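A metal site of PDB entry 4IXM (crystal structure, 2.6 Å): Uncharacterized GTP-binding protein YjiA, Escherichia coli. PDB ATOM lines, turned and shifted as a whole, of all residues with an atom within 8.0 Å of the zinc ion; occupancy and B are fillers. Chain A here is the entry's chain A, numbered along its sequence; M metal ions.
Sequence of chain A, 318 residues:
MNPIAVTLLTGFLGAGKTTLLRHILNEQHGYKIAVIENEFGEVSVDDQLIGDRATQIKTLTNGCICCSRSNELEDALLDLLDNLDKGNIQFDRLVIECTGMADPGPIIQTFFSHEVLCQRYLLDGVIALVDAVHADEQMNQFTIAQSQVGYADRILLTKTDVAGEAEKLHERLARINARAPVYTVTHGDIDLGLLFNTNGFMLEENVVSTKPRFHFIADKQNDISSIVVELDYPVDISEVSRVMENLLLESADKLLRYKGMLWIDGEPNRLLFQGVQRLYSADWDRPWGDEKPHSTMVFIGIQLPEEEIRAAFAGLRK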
ATOM      1  N   LEU A  21      -8.328  27.290 -25.696  1.00  0.00           N
ATOM      2  CA  LEU A  21      -7.408  26.279 -25.208  1.00  0.00           C
ATOM      3  C   LEU A  21      -8.099  24.929 -25.056  1.00  0.00           C
ATOM      4  O   LEU A  21      -7.514  23.883 -25.317  1.00  0.00           O
ATOM      5  CB  LEU A  21      -6.807  26.704 -23.868  1.00  0.00           C
ATOM      6  CG  LEU A  21      -5.425  27.362 -23.888  1.00  0.00           C
ATOM      7  CD1 LEU A  21      -5.347  28.451 -24.934  1.00  0.00           C
ATOM      8  CD2 LEU A  21      -5.072  27.904 -22.510  1.00  0.00           C
ATOM      9  N   LEU A  25      -6.949  21.296 -27.023  1.00  0.00           N
ATOM     10  CA  LEU A  25      -6.525  20.132 -26.249  1.00  0.00           C
ATOM     11  C   LEU A  25      -7.484  18.953 -26.358  1.00  0.00           C
ATOM     12  O   LEU A  25      -7.083  17.798 -26.228  1.00  0.00           O
ATOM     13  CB  LEU A  25      -6.331  20.520 -24.781  1.00  0.00           C
ATOM     14  CG  LEU A  25      -5.320  21.642 -24.520  1.00  0.00           C
ATOM     15  CD1 LEU A  25      -5.442  22.155 -23.097  1.00  0.00           C
ATOM     16  CD2 LEU A  25      -3.911  21.159 -24.815  1.00  0.00           C
ATOM     17  N   VAL A  35       1.076  22.156 -26.455  1.00  0.00           N
ATOM     18  CA  VAL A  35       0.622  23.353 -25.760  1.00  0.00           C
ATOM     19  C   VAL A  35       1.306  23.542 -24.405  1.00  0.00           C
ATOM     20  O   VAL A  35       1.328  22.624 -23.582  1.00  0.00           O
ATOM     21  CB  VAL A  35      -0.918  23.337 -25.543  1.00  0.00           C
ATOM     22  CG1 VAL A  35      -1.351  24.535 -24.711  1.00  0.00           C
ATOM     23  CG2 VAL A  35      -1.641  23.320 -26.879  1.00  0.00           C
ATOM     24  N   ILE A  36       1.852  24.727 -24.193  1.00  0.00           N
ATOM     25  CA  ILE A  36       2.347  25.123 -22.874  1.00  0.00           C
ATOM     26  C   ILE A  36       1.401  26.155 -22.282  1.00  0.00           C
ATOM     27  O   ILE A  36       1.313  27.295 -22.762  1.00  0.00           O
ATOM     28  CB  ILE A  36       3.765  25.702 -22.949  1.00  0.00           C
ATOM     29  CG1 ILE A  36       4.756  24.630 -23.427  1.00  0.00           C
ATOM     30  CG2 ILE A  36       4.194  26.255 -21.599  1.00  0.00           C
ATOM     31  CD1 ILE A  36       6.200  25.076 -23.389  1.00  0.00           C
ATOM     32  N   GLU A  37       0.681  25.761 -21.237  1.00  0.00           N
ATOM     33  CA  GLU A  37      -0.333  26.625 -20.648  1.00  0.00           C
ATOM     34  C   GLU A  37      -0.172  26.738 -19.135  1.00  0.00           C
ATOM     35  O   GLU A  37       0.643  26.052 -18.532  1.00  0.00           O
ATOM     36  CB  GLU A  37      -1.735  26.108 -20.987  1.00  0.00           C
ATOM     37  CG  GLU A  37      -1.997  24.698 -20.485  1.00  0.00           C
ATOM     38  CD  GLU A  37      -3.481  24.354 -20.462  1.00  0.00           C
ATOM     39  OE1 GLU A  37      -3.814  23.150 -20.376  1.00  0.00           O
ATOM     40  OE2 GLU A  37      -4.316  25.286 -20.521  1.00  0.00           O
ATOM     41  N   ASN A  38      -0.971  27.614 -18.539  1.00  0.00           N
ATOM     42  CA  ASN A  38      -0.921  27.851 -17.104  1.00  0.00           C
ATOM     43  C   ASN A  38      -1.911  26.984 -16.348  1.00  0.00           C
ATOM     44  O   ASN A  38      -1.654  26.571 -15.214  1.00  0.00           O
ATOM     45  CB  ASN A  38      -1.160  29.331 -16.790  1.00  0.00           C
ATOM     46  CG  ASN A  38      -0.184  30.245 -17.506  1.00  0.00           C
ATOM     47  OD1 ASN A  38       0.971  29.882 -17.748  1.00  0.00           O
ATOM     48  ND2 ASN A  38      -0.646  31.447 -17.842  1.00  0.00           N
ATOM     49  N   GLU A  39      -3.052  26.702 -16.977  1.00  0.00           N
ATOM     50  CA  GLU A  39      -4.118  25.958 -16.321  1.00  0.00           C
ATOM     51  C   GLU A  39      -4.099  24.473 -16.691  1.00  0.00           C
ATOM     52  O   GLU A  39      -3.030  23.854 -16.773  1.00  0.00           O
ATOM     53  CB  GLU A  39      -5.493  26.568 -16.628  1.00  0.00           C
ATOM     54  N   PHE A  40      -5.279  23.902 -16.901  1.00  0.00           N
ATOM     55  CA  PHE A  40      -5.431  22.472 -17.081  1.00  0.00           C
ATOM     56  C   PHE A  40      -6.761  22.253 -17.801  1.00  0.00           C
ATOM     57  O   PHE A  40      -7.783  21.977 -17.174  1.00  0.00           O
ATOM     58  CB  PHE A  40      -5.426  21.773 -15.705  1.00  0.00           C
ATOM     59  CG  PHE A  40      -5.582  20.280 -15.770  1.00  0.00           C
ATOM     60  CD1 PHE A  40      -4.484  19.463 -15.979  1.00  0.00           C
ATOM     61  CD2 PHE A  40      -6.818  19.679 -15.564  1.00  0.00           C
ATOM     62  CE1 PHE A  40      -4.613  18.093 -16.022  1.00  0.00           C
ATOM     63  CE2 PHE A  40      -6.957  18.299 -15.609  1.00  0.00           C
ATOM     64  CZ  PHE A  40      -5.852  17.508 -15.834  1.00  0.00           C
ATOM     65  N   GLY A  41      -6.746  22.412 -19.123  1.00  0.00           N
ATOM     66  CA  GLY A  41      -7.953  22.348 -19.910  1.00  0.00           C
ATOM     67  C   GLY A  41      -8.253  20.977 -20.460  1.00  0.00           C
ATOM     68  O   GLY A  41      -9.417  20.590 -20.590  1.00  0.00           O
ATOM     69  N   GLU A  42      -7.204  20.227 -20.790  1.00  0.00           N
ATOM     70  CA  GLU A  42      -7.361  18.877 -21.315  1.00  0.00           C
ATOM     71  C   GLU A  42      -8.039  17.958 -20.299  1.00  0.00           C
ATOM     72  O   GLU A  42      -7.912  18.143 -19.096  1.00  0.00           O
ATOM     73  CB  GLU A  42      -6.015  18.292 -21.742  1.00  0.00           C
ATOM     74  CG  GLU A  42      -4.803  19.064 -21.232  1.00  0.00           C
ATOM     75  CD  GLU A  42      -4.591  18.932 -19.741  1.00  0.00           C
ATOM     76  OE1 GLU A  42      -5.047  17.927 -19.163  1.00  0.00           O
ATOM     77  OE2 GLU A  42      -3.980  19.841 -19.145  1.00  0.00           O
ATOM     78  N   VAL A  43      -8.767  16.967 -20.811  1.00  0.00           N
ATOM     79  CA  VAL A  43      -9.478  16.024 -19.953  1.00  0.00           C
ATOM     80  C   VAL A  43      -9.010  14.599 -20.200  1.00  0.00           C
ATOM     81  O   VAL A  43      -8.770  13.841 -19.256  1.00  0.00           O
ATOM     82  CB  VAL A  43     -11.005  16.100 -20.172  1.00  0.00           C
ATOM     83  N   VAL A  45      -6.235  12.596 -20.961  1.00  0.00           N
ATOM     84  CA  VAL A  45      -4.792  12.420 -21.025  1.00  0.00           C
ATOM     85  C   VAL A  45      -4.458  10.971 -21.363  1.00  0.00           C
ATOM     86  O   VAL A  45      -4.740  10.060 -20.584  1.00  0.00           O
ATOM     87  CB  VAL A  45      -4.113  12.799 -19.705  1.00  0.00           C
ATOM     88  CG1 VAL A  45      -2.607  12.641 -19.817  1.00  0.00           C
ATOM     89  CG2 VAL A  45      -4.476  14.237 -19.318  1.00  0.00           C
ATOM     90  N   LYS A  58       2.485  15.523 -21.379  1.00  0.00           N
ATOM     91  CA  LYS A  58       1.285  14.700 -21.524  1.00  0.00           C
ATOM     92  C   LYS A  58       0.814  14.576 -22.969  1.00  0.00           C
ATOM     93  O   LYS A  58       0.624  15.578 -23.654  1.00  0.00           O
ATOM     94  CB  LYS A  58       0.138  15.265 -20.676  1.00  0.00           C
ATOM     95  CG  LYS A  58       0.393  15.261 -19.177  1.00  0.00           C
ATOM     96  CD  LYS A  58      -0.816  15.787 -18.425  1.00  0.00           C
ATOM     97  CE  LYS A  58      -0.567  15.790 -16.924  1.00  0.00           C
ATOM     98  NZ  LYS A  58      -1.763  16.272 -16.175  1.00  0.00           N
ATOM     99  N   LEU A  60      -2.129  13.636 -25.548  1.00  0.00           N
ATOM    100  CA  LEU A  60      -3.587  13.642 -25.494  1.00  0.00           C
ATOM    101  C   LEU A  60      -4.224  12.697 -26.512  1.00  0.00           C
ATOM    102  O   LEU A  60      -3.556  12.213 -27.420  1.00  0.00           O
ATOM    103  CB  LEU A  60      -4.110  15.064 -25.689  1.00  0.00           C
ATOM    104  CG  LEU A  60      -3.496  16.129 -24.781  1.00  0.00           C
ATOM    105  CD1 LEU A  60      -4.077  17.493 -25.091  1.00  0.00           C
ATOM    106  CD2 LEU A  60      -3.699  15.776 -23.321  1.00  0.00           C
ATOM    107  N   ILE A  65      -0.323  17.523 -27.628  1.00  0.00           N
ATOM    108  CA  ILE A  65       0.521  17.354 -26.446  1.00  0.00           C
ATOM    109  C   ILE A  65       0.300  18.518 -25.487  1.00  0.00           C
ATOM    110  O   ILE A  65       0.244  19.674 -25.905  1.00  0.00           O
ATOM    111  CB  ILE A  65       2.015  17.310 -26.836  1.00  0.00           C
ATOM    112  CG1 ILE A  65       2.253  16.271 -27.934  1.00  0.00           C
ATOM    113  CG2 ILE A  65       2.879  17.040 -25.628  1.00  0.00           C
ATOM    114  CD1 ILE A  65       2.030  14.842 -27.488  1.00  0.00           C
ATOM    115  N   CYS A  66       0.192  18.216 -24.198  1.00  0.00           N
ATOM    116  CA  CYS A  66       0.131  19.250 -23.177  1.00  0.00           C
ATOM    117  C   CYS A  66       1.403  19.226 -22.346  1.00  0.00           C
ATOM    118  O   CYS A  66       1.815  18.177 -21.850  1.00  0.00           O
ATOM    119  CB  CYS A  66      -1.101  19.088 -22.295  1.00  0.00           C
ATOM    120  SG  CYS A  66      -1.511  20.566 -21.339  1.00  0.00           S
ATOM    121  N   CYS A  67       2.016  20.401 -22.174  1.00  0.00           N
ATOM    122  CA  CYS A  67       3.322  20.487 -21.536  1.00  0.00           C
ATOM    123  C   CYS A  67       3.341  21.556 -20.443  1.00  0.00           C
ATOM    124  O   CYS A  67       2.691  22.588 -20.561  1.00  0.00           O
ATOM    125  CB  CYS A  67       4.395  20.791 -22.586  1.00  0.00           C
ATOM    126  SG  CYS A  67       6.072  20.859 -21.943  1.00  0.00           S
ATOM    127  N   SER A  68       4.093  21.283 -19.386  1.00  0.00           N
ATOM    128  CA  SER A  68       4.249  22.230 -18.294  1.00  0.00           C
ATOM    129  C   SER A  68       5.570  22.989 -18.442  1.00  0.00           C
ATOM    130  O   SER A  68       6.446  22.576 -19.200  1.00  0.00           O
ATOM    131  CB  SER A  68       4.211  21.509 -16.945  1.00  0.00           C
ATOM    132  OG  SER A  68       5.306  20.621 -16.822  1.00  0.00           O
ATOM    133  N   GLU A  97       1.104  29.871 -24.006  1.00  0.00           N
ATOM    134  CA  GLU A  97       0.224  30.851 -23.400  1.00  0.00           C
ATOM    135  C   GLU A  97       1.017  31.878 -22.605  1.00  0.00           C
ATOM    136  O   GLU A  97       1.776  31.536 -21.702  1.00  0.00           O
ATOM    137  CB  GLU A  97      -0.799  30.170 -22.482  1.00  0.00           C
ATOM    138  CG  GLU A  97      -1.737  31.139 -21.783  1.00  0.00           C
ATOM    139  CD  GLU A  97      -2.571  30.466 -20.714  1.00  0.00           C
ATOM    140  OE1 GLU A  97      -2.685  29.222 -20.743  1.00  0.00           O
ATOM    141  OE2 GLU A  97      -3.105  31.177 -19.834  1.00  0.00           O
HETATM  142 ZN    ZN M   1      -2.724  21.501 -19.589  1.00  0.00          ZN
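OE1 of Glu 37 binds the zinc ion, at 2.1 Å. The zinc ion is bound by OE2 of Glu 42 (2.1 Å). The side-chain sulfur (SG) of Cys 66 is bound to the zinc ion (2.3 Å). The zinc ion has three donor atoms within binding distance.
The side-chain carboxylate of Glu 37 sits close to the backbone NH of Gly 41. N of Cys 66 sits at hydrogen-bond distance from O of Lys 58, 2.7 Å away.
O of Glu 39 touches the zinc ion, at 3.7 Å. Phe 40 touches the zinc ion. Within 4 Å of the zinc ion: Glu 37, Glu 39, Phe 40, Glu 42 and Cys 66. The nearest printed residue that does not touch the zinc ion is Gly 41 (4.2 Å).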
